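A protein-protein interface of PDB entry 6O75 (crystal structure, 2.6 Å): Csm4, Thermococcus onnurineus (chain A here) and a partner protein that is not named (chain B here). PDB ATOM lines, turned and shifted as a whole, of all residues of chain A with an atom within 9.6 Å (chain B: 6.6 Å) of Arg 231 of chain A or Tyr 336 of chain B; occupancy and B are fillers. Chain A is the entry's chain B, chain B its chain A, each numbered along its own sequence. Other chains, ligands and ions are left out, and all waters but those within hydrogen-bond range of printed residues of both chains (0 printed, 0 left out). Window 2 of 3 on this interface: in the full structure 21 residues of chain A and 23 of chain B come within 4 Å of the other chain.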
ATOM      1  N   ARG A  20     -10.158  17.002  13.057  1.00  0.00           N
ATOM      2  CA  ARG A  20      -9.069  16.338  13.810  1.00  0.00           C
ATOM      3  C   ARG A  20      -8.792  14.967  13.182  1.00  0.00           C
ATOM      4  O   ARG A  20      -9.508  14.581  12.240  1.00  0.00           O
ATOM      5  CB  ARG A  20      -9.320  16.382  15.322  1.00  0.00           C
ATOM      6  CG  ARG A  20     -10.741  16.135  15.808  1.00  0.00           C
ATOM      7  CD  ARG A  20     -11.245  17.115  16.870  1.00  0.00           C
ATOM      8  NE  ARG A  20     -10.233  17.782  17.691  1.00  0.00           N
ATOM      9  CZ  ARG A  20     -10.490  18.680  18.650  1.00  0.00           C
ATOM     10  NH1 ARG A  20     -11.735  19.023  18.942  1.00  0.00           N
ATOM     11  NH2 ARG A  20      -9.492  19.230  19.325  1.00  0.00           N
ATOM     12  N   ASP A  22      -8.959  11.768  13.733  1.00  0.00           N
ATOM     13  CA  ASP A  22     -10.004  10.708  13.666  1.00  0.00           C
ATOM     14  C   ASP A  22     -10.944  11.015  12.490  1.00  0.00           C
ATOM     15  O   ASP A  22     -11.090  10.142  11.625  1.00  0.00           O
ATOM     16  CB  ASP A  22     -10.739  10.517  15.000  1.00  0.00           C
ATOM     17  CG  ASP A  22     -11.569  11.710  15.448  1.00  0.00           C
ATOM     18  OD1 ASP A  22     -10.966  12.792  15.668  1.00  0.00           O
ATOM     19  OD2 ASP A  22     -12.813  11.555  15.564  1.00  0.00           O
ATOM     20  N   ASN A 217      -5.185  13.970  17.802  1.00  0.00           N
ATOM     21  CA  ASN A 217      -6.024  13.428  18.899  1.00  0.00           C
ATOM     22  C   ASN A 217      -5.830  11.912  18.893  1.00  0.00           C
ATOM     23  O   ASN A 217      -5.823  11.336  17.799  1.00  0.00           O
ATOM     24  CB  ASN A 217      -7.482  13.879  18.787  1.00  0.00           C
ATOM     25  CG  ASN A 217      -8.197  13.375  17.551  1.00  0.00           C
ATOM     26  OD1 ASN A 217      -7.635  13.338  16.459  1.00  0.00           O
ATOM     27  ND2 ASN A 217      -9.453  13.002  17.719  1.00  0.00           N
ATOM     28  N   ALA A 218      -5.623  11.306  20.065  1.00  0.00           N
ATOM     29  CA  ALA A 218      -5.156   9.909  20.214  1.00  0.00           C
ATOM     30  C   ALA A 218      -5.978   9.151  21.262  1.00  0.00           C
ATOM     31  O   ALA A 218      -6.482   9.778  22.216  1.00  0.00           O
ATOM     32  CB  ALA A 218      -3.691   9.908  20.570  1.00  0.00           C
ATOM     33  N   LEU A 219      -6.103   7.836  21.052  1.00  0.00           N
ATOM     34  CA  LEU A 219      -6.554   6.826  22.043  1.00  0.00           C
ATOM     35  C   LEU A 219      -5.304   6.224  22.669  1.00  0.00           C
ATOM     36  O   LEU A 219      -4.639   5.399  22.050  1.00  0.00           O
ATOM     37  CB  LEU A 219      -7.370   5.750  21.323  1.00  0.00           C
ATOM     38  CG  LEU A 219      -8.585   6.257  20.557  1.00  0.00           C
ATOM     39  CD1 LEU A 219      -9.115   5.180  19.626  1.00  0.00           C
ATOM     40  CD2 LEU A 219      -9.670   6.725  21.511  1.00  0.00           C
ATOM     41  N   TRP A 227      -2.410  16.238  29.650  1.00  0.00           N
ATOM     42  CA  TRP A 227      -3.461  15.974  28.636  1.00  0.00           C
ATOM     43  C   TRP A 227      -4.725  16.793  28.898  1.00  0.00           C
ATOM     44  O   TRP A 227      -4.965  17.182  30.057  1.00  0.00           O
ATOM     45  CB  TRP A 227      -3.782  14.479  28.602  1.00  0.00           C
ATOM     46  CG  TRP A 227      -4.574  13.967  29.767  1.00  0.00           C
ATOM     47  CD1 TRP A 227      -5.932  13.983  29.901  1.00  0.00           C
ATOM     48  CD2 TRP A 227      -4.067  13.300  30.940  1.00  0.00           C
ATOM     49  NE1 TRP A 227      -6.303  13.397  31.080  1.00  0.00           N
ATOM     50  CE2 TRP A 227      -5.182  12.964  31.737  1.00  0.00           C
ATOM     51  CE3 TRP A 227      -2.787  12.956  31.398  1.00  0.00           C
ATOM     52  CZ2 TRP A 227      -5.050  12.292  32.954  1.00  0.00           C
ATOM     53  CZ3 TRP A 227      -2.658  12.292  32.599  1.00  0.00           C
ATOM     54  CH2 TRP A 227      -3.776  11.966  33.368  1.00  0.00           C
ATOM     55  N   ARG A 228      -5.481  17.037  27.826  1.00  0.00           N
ATOM     56  CA  ARG A 228      -6.895  17.478  27.847  1.00  0.00           C
ATOM     57  C   ARG A 228      -7.741  16.344  27.265  1.00  0.00           C
ATOM     58  O   ARG A 228      -7.437  15.871  26.157  1.00  0.00           O
ATOM     59  CB  ARG A 228      -7.087  18.768  27.047  1.00  0.00           C
ATOM     60  CG  ARG A 228      -6.458  19.998  27.682  1.00  0.00           C
ATOM     61  CD  ARG A 228      -7.160  21.284  27.276  1.00  0.00           C
ATOM     62  NE  ARG A 228      -7.613  21.275  25.886  1.00  0.00           N
ATOM     63  CZ  ARG A 228      -6.830  21.427  24.814  1.00  0.00           C
ATOM     64  NH1 ARG A 228      -7.361  21.399  23.603  1.00  0.00           N
ATOM     65  NH2 ARG A 228      -5.525  21.601  24.949  1.00  0.00           N
ATOM     66  N   LEU A 229      -8.760  15.913  27.999  1.00  0.00           N
ATOM     67  CA  LEU A 229      -9.741  14.916  27.516  1.00  0.00           C
ATOM     68  C   LEU A 229     -10.590  15.548  26.416  1.00  0.00           C
ATOM     69  O   LEU A 229     -10.840  16.765  26.462  1.00  0.00           O
ATOM     70  CB  LEU A 229     -10.603  14.438  28.685  1.00  0.00           C
ATOM     71  CG  LEU A 229      -9.850  13.613  29.723  1.00  0.00           C
ATOM     72  CD1 LEU A 229     -10.751  13.295  30.903  1.00  0.00           C
ATOM     73  CD2 LEU A 229      -9.286  12.337  29.099  1.00  0.00           C
ATOM     74  N   LEU A 230     -11.008  14.711  25.473  1.00  0.00           N
ATOM     75  CA  LEU A 230     -11.803  15.086  24.286  1.00  0.00           C
ATOM     76  C   LEU A 230     -12.887  14.019  24.109  1.00  0.00           C
ATOM     77  O   LEU A 230     -12.548  12.897  23.670  1.00  0.00           O
ATOM     78  CB  LEU A 230     -10.833  15.157  23.104  1.00  0.00           C
ATOM     79  CG  LEU A 230     -11.383  15.722  21.802  1.00  0.00           C
ATOM     80  CD1 LEU A 230     -12.009  17.092  22.016  1.00  0.00           C
ATOM     81  CD2 LEU A 230     -10.273  15.794  20.764  1.00  0.00           C
ATOM     82  N   ARG A 231     -14.123  14.350  24.501  1.00  0.00           N
ATOM     83  CA  ARG A 231     -15.296  13.433  24.525  1.00  0.00           C
ATOM     84  C   ARG A 231     -15.932  13.372  23.127  1.00  0.00           C
ATOM     85  O   ARG A 231     -16.235  14.446  22.568  1.00  0.00           O
ATOM     86  CB  ARG A 231     -16.297  13.921  25.579  1.00  0.00           C
ATOM     87  CG  ARG A 231     -17.416  12.941  25.900  1.00  0.00           C
ATOM     88  CD  ARG A 231     -16.964  11.805  26.798  1.00  0.00           C
ATOM     89  NE  ARG A 231     -17.980  10.764  26.877  1.00  0.00           N
ATOM     90  CZ  ARG A 231     -17.860   9.627  27.557  1.00  0.00           C
ATOM     91  NH1 ARG A 231     -16.755   9.363  28.238  1.00  0.00           N
ATOM     92  NH2 ARG A 231     -18.853   8.753  27.551  1.00  0.00           N
ATOM     93  N   LYS A 232     -16.116  12.162  22.585  1.00  0.00           N
ATOM     94  CA  LYS A 232     -16.765  11.913  21.267  1.00  0.00           C
ATOM     95  C   LYS A 232     -17.507  10.572  21.315  1.00  0.00           C
ATOM     96  O   LYS A 232     -18.596  10.505  20.714  1.00  0.00           O
ATOM     97  CB  LYS A 232     -15.729  11.920  20.137  1.00  0.00           C
ATOM     98  CG  LYS A 232     -15.223  13.298  19.724  1.00  0.00           C
ATOM     99  CD  LYS A 232     -14.395  13.279  18.454  1.00  0.00           C
ATOM    100  CE  LYS A 232     -14.014  14.662  17.965  1.00  0.00           C
ATOM    101  NZ  LYS A 232     -13.546  14.634  16.559  1.00  0.00           N
ATOM    102  N   ARG A 243     -19.323   6.145  22.274  1.00  0.00           N
ATOM    103  CA  ARG A 243     -18.572   7.353  22.716  1.00  0.00           C
ATOM    104  C   ARG A 243     -17.133   6.958  23.072  1.00  0.00           C
ATOM    105  O   ARG A 243     -16.963   6.019  23.877  1.00  0.00           O
ATOM    106  CB  ARG A 243     -19.271   8.022  23.905  1.00  0.00           C
ATOM    107  CG  ARG A 243     -20.567   8.735  23.546  1.00  0.00           C
ATOM    108  CD  ARG A 243     -21.128   9.527  24.713  1.00  0.00           C
ATOM    109  NE  ARG A 243     -22.259  10.372  24.342  1.00  0.00           N
ATOM    110  CZ  ARG A 243     -22.174  11.554  23.728  1.00  0.00           C
ATOM    111  NH1 ARG A 243     -20.999  12.058  23.385  1.00  0.00           N
ATOM    112  NH2 ARG A 243     -23.277  12.229  23.452  1.00  0.00           N
ATOM    113  N   MET A 244     -16.151   7.657  22.491  1.00  0.00           N
ATOM    114  CA  MET A 244     -14.690   7.418  22.662  1.00  0.00           C
ATOM    115  C   MET A 244     -14.083   8.511  23.553  1.00  0.00           C
ATOM    116  O   MET A 244     -14.498   9.681  23.417  1.00  0.00           O
ATOM    117  CB  MET A 244     -13.974   7.455  21.305  1.00  0.00           C
ATOM    118  CG  MET A 244     -14.496   6.458  20.283  1.00  0.00           C
ATOM    119  SD  MET A 244     -14.564   4.755  20.887  1.00  0.00           S
ATOM    120  CE  MET A 244     -12.983   4.593  21.719  1.00  0.00           C
ATOM    121  N   THR A 245     -13.117   8.153  24.406  1.00  0.00           N
ATOM    122  CA  THR A 245     -12.326   9.122  25.215  1.00  0.00           C
ATOM    123  C   THR A 245     -10.955   9.321  24.555  1.00  0.00           C
ATOM    124  O   THR A 245     -10.092   8.425  24.663  1.00  0.00           O
ATOM    125  CB  THR A 245     -12.234   8.704  26.687  1.00  0.00           C
ATOM    126  OG1 THR A 245     -11.700   7.385  26.772  1.00  0.00           O
ATOM    127  CG2 THR A 245     -13.575   8.758  27.387  1.00  0.00           C
ATOM    128  N   PHE A 246     -10.777  10.469  23.896  1.00  0.00           N
ATOM    129  CA  PHE A 246      -9.529  10.881  23.207  1.00  0.00           C
ATOM    130  C   PHE A 246      -8.719  11.851  24.078  1.00  0.00           C
ATOM    131  O   PHE A 246      -9.284  12.663  24.836  1.00  0.00           O
ATOM    132  CB  PHE A 246      -9.838  11.557  21.869  1.00  0.00           C
ATOM    133  CG  PHE A 246     -10.148  10.631  20.722  1.00  0.00           C
ATOM    134  CD1 PHE A 246      -9.130  10.082  19.959  1.00  0.00           C
ATOM    135  CD2 PHE A 246     -11.460  10.352  20.368  1.00  0.00           C
ATOM    136  CE1 PHE A 246      -9.419   9.259  18.882  1.00  0.00           C
ATOM    137  CE2 PHE A 246     -11.746   9.524  19.294  1.00  0.00           C
ATOM    138  CZ  PHE A 246     -10.726   8.980  18.554  1.00  0.00           C
ATOM    139  N   ILE A 247      -7.401  11.739  23.947  1.00  0.00           N
ATOM    140  CA  ILE A 247      -6.371  12.739  24.349  1.00  0.00           C
ATOM    141  C   ILE A 247      -6.325  13.805  23.245  1.00  0.00           C
ATOM    142  O   ILE A 247      -6.203  13.428  22.075  1.00  0.00           O
ATOM    143  CB  ILE A 247      -5.033  11.991  24.539  1.00  0.00           C
ATOM    144  CG1 ILE A 247      -4.852  11.526  25.981  1.00  0.00           C
ATOM    145  CG2 ILE A 247      -3.828  12.781  24.076  1.00  0.00           C
ATOM    146  CD1 ILE A 247      -3.679  10.593  26.128  1.00  0.00           C
ATOM    147  N   ALA A 248      -6.425  15.089  23.587  1.00  0.00           N
ATOM    148  CA  ALA A 248      -6.416  16.206  22.613  1.00  0.00           C
ATOM    149  C   ALA A 248      -5.014  16.406  22.022  1.00  0.00           C
ATOM    150  O   ALA A 248      -4.027  15.944  22.619  1.00  0.00           O
ATOM    151  CB  ALA A 248      -6.892  17.478  23.272  1.00  0.00           C
ATOM    152  N   ALA B 331     -14.217  10.636  45.260  1.00  0.00           N
ATOM    153  CA  ALA B 331     -14.949  11.845  44.817  1.00  0.00           C
ATOM    154  C   ALA B 331     -14.865  11.950  43.289  1.00  0.00           C
ATOM    155  O   ALA B 331     -15.918  12.128  42.649  1.00  0.00           O
ATOM    156  CB  ALA B 331     -14.397  13.074  45.493  1.00  0.00           C
ATOM    157  N   VAL B 332     -13.661  11.820  42.726  1.00  0.00           N
ATOM    158  CA  VAL B 332     -13.423  11.889  41.254  1.00  0.00           C
ATOM    159  C   VAL B 332     -14.199  10.757  40.565  1.00  0.00           C
ATOM    160  O   VAL B 332     -14.894  11.042  39.574  1.00  0.00           O
ATOM    161  CB  VAL B 332     -11.923  11.827  40.923  1.00  0.00           C
ATOM    162  CG1 VAL B 332     -11.691  11.585  39.437  1.00  0.00           C
ATOM    163  CG2 VAL B 332     -11.201  13.087  41.379  1.00  0.00           C
ATOM    164  N   GLU B 333     -14.070   9.522  41.062  1.00  0.00           N
ATOM    165  CA  GLU B 333     -14.715   8.315  40.479  1.00  0.00           C
ATOM    166  C   GLU B 333     -16.220   8.568  40.406  1.00  0.00           C
ATOM    167  O   GLU B 333     -16.834   8.191  39.393  1.00  0.00           O
ATOM    168  CB  GLU B 333     -14.386   7.056  41.288  1.00  0.00           C
ATOM    169  CG  GLU B 333     -13.076   6.404  40.870  1.00  0.00           C
ATOM    170  CD  GLU B 333     -12.424   5.486  41.893  1.00  0.00           C
ATOM    171  OE1 GLU B 333     -13.137   5.009  42.801  1.00  0.00           O
ATOM    172  OE2 GLU B 333     -11.197   5.250  41.778  1.00  0.00           O
ATOM    173  N   TRP B 334     -16.780   9.212  41.431  1.00  0.00           N
ATOM    174  CA  TRP B 334     -18.231   9.530  41.498  1.00  0.00           C
ATOM    175  C   TRP B 334     -18.580  10.599  40.457  1.00  0.00           C
ATOM    176  O   TRP B 334     -19.624  10.461  39.821  1.00  0.00           O
ATOM    177  CB  TRP B 334     -18.640   9.974  42.904  1.00  0.00           C
ATOM    178  CG  TRP B 334     -20.101  10.288  43.004  1.00  0.00           C
ATOM    179  CD1 TRP B 334     -21.116   9.413  43.256  1.00  0.00           C
ATOM    180  CD2 TRP B 334     -20.717  11.577  42.844  1.00  0.00           C
ATOM    181  NE1 TRP B 334     -22.318  10.067  43.269  1.00  0.00           N
ATOM    182  CE2 TRP B 334     -22.104  11.396  43.025  1.00  0.00           C
ATOM    183  CE3 TRP B 334     -20.234  12.863  42.579  1.00  0.00           C
ATOM    184  CZ2 TRP B 334     -23.007  12.453  42.937  1.00  0.00           C
ATOM    185  CZ3 TRP B 334     -21.128  13.908  42.492  1.00  0.00           C
ATOM    186  CH2 TRP B 334     -22.495  13.702  42.669  1.00  0.00           C
ATOM    187  N   LEU B 335     -17.746  11.632  40.312  1.00  0.00           N
ATOM    188  CA  LEU B 335     -17.991  12.744  39.356  1.00  0.00           C
ATOM    189  C   LEU B 335     -18.018  12.171  37.940  1.00  0.00           C
ATOM    190  O   LEU B 335     -18.908  12.572  37.166  1.00  0.00           O
ATOM    191  CB  LEU B 335     -16.906  13.819  39.493  1.00  0.00           C
ATOM    192  CG  LEU B 335     -16.991  14.701  40.738  1.00  0.00           C
ATOM    193  CD1 LEU B 335     -15.762  15.592  40.854  1.00  0.00           C
ATOM    194  CD2 LEU B 335     -18.258  15.540  40.723  1.00  0.00           C
ATOM    195  N   TYR B 336     -17.081  11.265  37.633  1.00  0.00           N
ATOM    196  CA  TYR B 336     -16.913  10.642  36.296  1.00  0.00           C
ATOM    197  C   TYR B 336     -18.155   9.821  35.952  1.00  0.00           C
ATOM    198  O   TYR B 336     -18.690  10.005  34.846  1.00  0.00           O
ATOM    199  CB  TYR B 336     -15.658   9.772  36.227  1.00  0.00           C
ATOM    200  CG  TYR B 336     -15.351   9.273  34.836  1.00  0.00           C
ATOM    201  CD1 TYR B 336     -15.872   8.073  34.372  1.00  0.00           C
ATOM    202  CD2 TYR B 336     -14.555  10.009  33.971  1.00  0.00           C
ATOM    203  CE1 TYR B 336     -15.601   7.612  33.093  1.00  0.00           C
ATOM    204  CE2 TYR B 336     -14.275   9.563  32.690  1.00  0.00           C
ATOM    205  CZ  TYR B 336     -14.798   8.359  32.248  1.00  0.00           C
ATOM    206  OH  TYR B 336     -14.517   7.915  30.988  1.00  0.00           O
ATOM    207  N   ARG B 337     -18.597   8.953  36.868  1.00  0.00           N
ATOM    208  CA  ARG B 337     -19.785   8.072  36.685  1.00  0.00           C
ATOM    209  C   ARG B 337     -21.056   8.921  36.540  1.00  0.00           C
ATOM    210  O   ARG B 337     -21.955   8.502  35.792  1.00  0.00           O
ATOM    211  CB  ARG B 337     -19.912   7.087  37.850  1.00  0.00           C
ATOM    212  CG  ARG B 337     -18.817   6.029  37.876  1.00  0.00           C
ATOM    213  CD  ARG B 337     -18.714   5.272  39.192  1.00  0.00           C
ATOM    214  NE  ARG B 337     -17.400   4.650  39.354  1.00  0.00           N
ATOM    215  CZ  ARG B 337     -17.087   3.732  40.268  1.00  0.00           C
ATOM    216  NH1 ARG B 337     -17.993   3.300  41.130  1.00  0.00           N
ATOM    217  NH2 ARG B 337     -15.858   3.242  40.313  1.00  0.00           N
ATOM    218  N   GLU B 338     -21.119  10.078  37.207  1.00  0.00           N
ATOM    219  CA  GLU B 338     -22.362  10.883  37.358  1.00  0.00           C
ATOM    220  C   GLU B 338     -22.507  11.901  36.217  1.00  0.00           C
ATOM    221  O   GLU B 338     -23.662  12.191  35.851  1.00  0.00           O
ATOM    222  CB  GLU B 338     -22.364  11.587  38.716  1.00  0.00           C
ATOM    223  CG  GLU B 338     -23.753  11.939  39.210  1.00  0.00           C
ATOM    224  CD  GLU B 338     -24.617  10.747  39.598  1.00  0.00           C
ATOM    225  OE1 GLU B 338     -25.857  10.912  39.661  1.00  0.00           O
ATOM    226  OE2 GLU B 338     -24.052   9.660  39.842  1.00  0.00           O
ATOM    227  N   PHE B 339     -21.402  12.445  35.690  1.00  0.00           N
ATOM    228  CA  PHE B 339     -21.412  13.597  34.744  1.00  0.00           C
ATOM    229  C   PHE B 339     -20.392  13.451  33.602  1.00  0.00           C
ATOM    230  O   PHE B 339     -20.216  14.441  32.861  1.00  0.00           O
ATOM    231  CB  PHE B 339     -21.121  14.889  35.509  1.00  0.00           C
ATOM    232  CG  PHE B 339     -22.001  15.121  36.709  1.00  0.00           C
ATOM    233  CD1 PHE B 339     -23.372  15.258  36.563  1.00  0.00           C
ATOM    234  CD2 PHE B 339     -21.458  15.220  37.978  1.00  0.00           C
ATOM    235  CE1 PHE B 339     -24.183  15.480  37.665  1.00  0.00           C
ATOM    236  CE2 PHE B 339     -22.268  15.445  39.079  1.00  0.00           C
ATOM    237  CZ  PHE B 339     -23.628  15.574  38.920  1.00  0.00           C
ATOM    238  N   GLU B 340     -19.753  12.283  33.451  1.00  0.00           N
ATOM    239  CA  GLU B 340     -18.704  12.014  32.423  1.00  0.00           C
ATOM    240  C   GLU B 340     -17.507  12.941  32.679  1.00  0.00           C
ATOM    241  O   GLU B 340     -17.220  13.223  33.861  1.00  0.00           O
ATOM    242  CB  GLU B 340     -19.279  12.197  31.013  1.00  0.00           C
ATOM    243  CG  GLU B 340     -20.657  11.588  30.824  1.00  0.00           C
ATOM    244  CD  GLU B 340     -21.601  12.445  29.999  1.00  0.00           C
ATOM    245  OE1 GLU B 340     -21.228  12.803  28.863  1.00  0.00           O
ATOM    246  OE2 GLU B 340     -22.699  12.767  30.502  1.00  0.00           O
ATOM    247  N   SER B 341     -16.844  13.410  31.618  1.00  0.00           N
ATOM    248  CA  SER B 341     -15.680  14.331  31.687  1.00  0.00           C
ATOM    249  C   SER B 341     -16.103  15.744  32.120  1.00  0.00           C
ATOM    250  O   SER B 341     -15.196  16.529  32.416  1.00  0.00           O
ATOM    251  CB  SER B 341     -14.944  14.370  30.364  1.00  0.00           C
ATOM    252  OG  SER B 341     -13.990  15.425  30.339  1.00  0.00           O
ATOM    253  N   LEU B 343     -17.606  17.639  34.770  1.00  0.00           N
ATOM    254  CA  LEU B 343     -17.143  18.250  36.043  1.00  0.00           C
ATOM    255  C   LEU B 343     -16.027  17.396  36.646  1.00  0.00           C
ATOM    256  O   LEU B 343     -16.263  16.197  36.873  1.00  0.00           O
ATOM    257  CB  LEU B 343     -18.320  18.386  37.014  1.00  0.00           C
ATOM    258  CG  LEU B 343     -18.030  19.195  38.279  1.00  0.00           C
ATOM    259  CD1 LEU B 343     -17.619  20.620  37.942  1.00  0.00           C
ATOM    260  CD2 LEU B 343     -19.230  19.199  39.216  1.00  0.00           C
ATOM    261  N   PHE B 385      -8.890  13.371  35.687  1.00  0.00           N
ATOM    262  CA  PHE B 385      -9.455  12.014  35.895  1.00  0.00           C
ATOM    263  C   PHE B 385      -8.346  10.952  35.842  1.00  0.00           C
ATOM    264  O   PHE B 385      -8.686   9.765  35.691  1.00  0.00           O
ATOM    265  CB  PHE B 385     -10.562  11.741  34.875  1.00  0.00           C
ATOM    266  CG  PHE B 385     -11.826  12.526  35.102  1.00  0.00           C
ATOM    267  CD1 PHE B 385     -12.696  12.183  36.123  1.00  0.00           C
ATOM    268  CD2 PHE B 385     -12.150  13.605  34.298  1.00  0.00           C
ATOM    269  CE1 PHE B 385     -13.863  12.902  36.335  1.00  0.00           C
ATOM    270  CE2 PHE B 385     -13.314  14.326  34.515  1.00  0.00           C
ATOM    271  CZ  PHE B 385     -14.171  13.970  35.528  1.00  0.00           C
ATOM    272  N   ILE B 388      -8.457   7.585  37.839  1.00  0.00           N
ATOM    273  CA  ILE B 388      -9.147   6.391  37.266  1.00  0.00           C
ATOM    274  C   ILE B 388      -8.191   5.734  36.264  1.00  0.00           C
ATOM    275  O   ILE B 388      -7.898   6.387  35.242  1.00  0.00           O
ATOM    276  CB  ILE B 388     -10.465   6.813  36.581  1.00  0.00           C
ATOM    277  CG1 ILE B 388     -11.389   7.574  37.535  1.00  0.00           C
ATOM    278  CG2 ILE B 388     -11.168   5.616  35.953  1.00  0.00           C
ATOM    279  CD1 ILE B 388     -12.475   8.363  36.838  1.00  0.00           C
ATOM    280  N   GLY B 390      -9.013   2.982  34.708  1.00  0.00           N
ATOM    281  CA  GLY B 390      -9.977   2.456  33.719  1.00  0.00           C
ATOM    282  C   GLY B 390     -10.355   3.481  32.656  1.00  0.00           C
ATOM    283  O   GLY B 390     -11.277   3.195  31.866  1.00  0.00           O
ATOM    284  N   LEU B 391      -9.660   4.622  32.612  1.00  0.00           N
ATOM    285  CA  LEU B 391     -10.025   5.802  31.784  1.00  0.00           C
ATOM    286  C   LEU B 391      -9.733   5.532  30.304  1.00  0.00           C
ATOM    287  O   LEU B 391     -10.565   5.920  29.461  1.00  0.00           O
ATOM    288  CB  LEU B 391      -9.235   7.016  32.281  1.00  0.00           C
ATOM    289  CG  LEU B 391      -9.485   8.320  31.523  1.00  0.00           C
ATOM    290  CD1 LEU B 391     -10.949   8.725  31.605  1.00  0.00           C
ATOM    291  CD2 LEU B 391      -8.587   9.429  32.049  1.00  0.00           C
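The backbone carbonyl oxygen of Leu 391 of chain B sits at hydrogen-bond distance from the side-chain hydroxyl of Thr 245 of chain A, 3.3 Å away.
Leu 229 of chain A touches Ser 341 of chain B (CB to OG, 3.9 Å).
CD1 of Leu 229 of chain A touches CD2 of Phe 385 of chain B, at 3.7 Å.
Arg 231 of chain A touches Tyr 336 of chain B.
Tyr 336 of chain B touches Thr 245 of chain A (OH to CG2, 3.8 Å).
Of chain B, only Tyr 336 (3.8 Å) comes within 4 Å of Arg 231 of chain A.
Val 332 of chain B touches none of the printed residues of chain A.
Tyr 336 of chain B touches two residues of chain A.
Of the printed residues of chain A, Ser 341 of chain B touches Leu 229 (3.9 Å).
Printed residues of chain A within 4 Å of Phe 385 of chain B: Leu 229 (3.7 Å).
The nearest printed residue of chain B that does not touch Leu 229 of chain A is Leu 391 of chain B (4.2 Å).
Hydrophobic or aromatic side chains of chain A that line the printed part of chain B: Leu 229.
Among the printed residues, 5 pairs touch across the chains.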
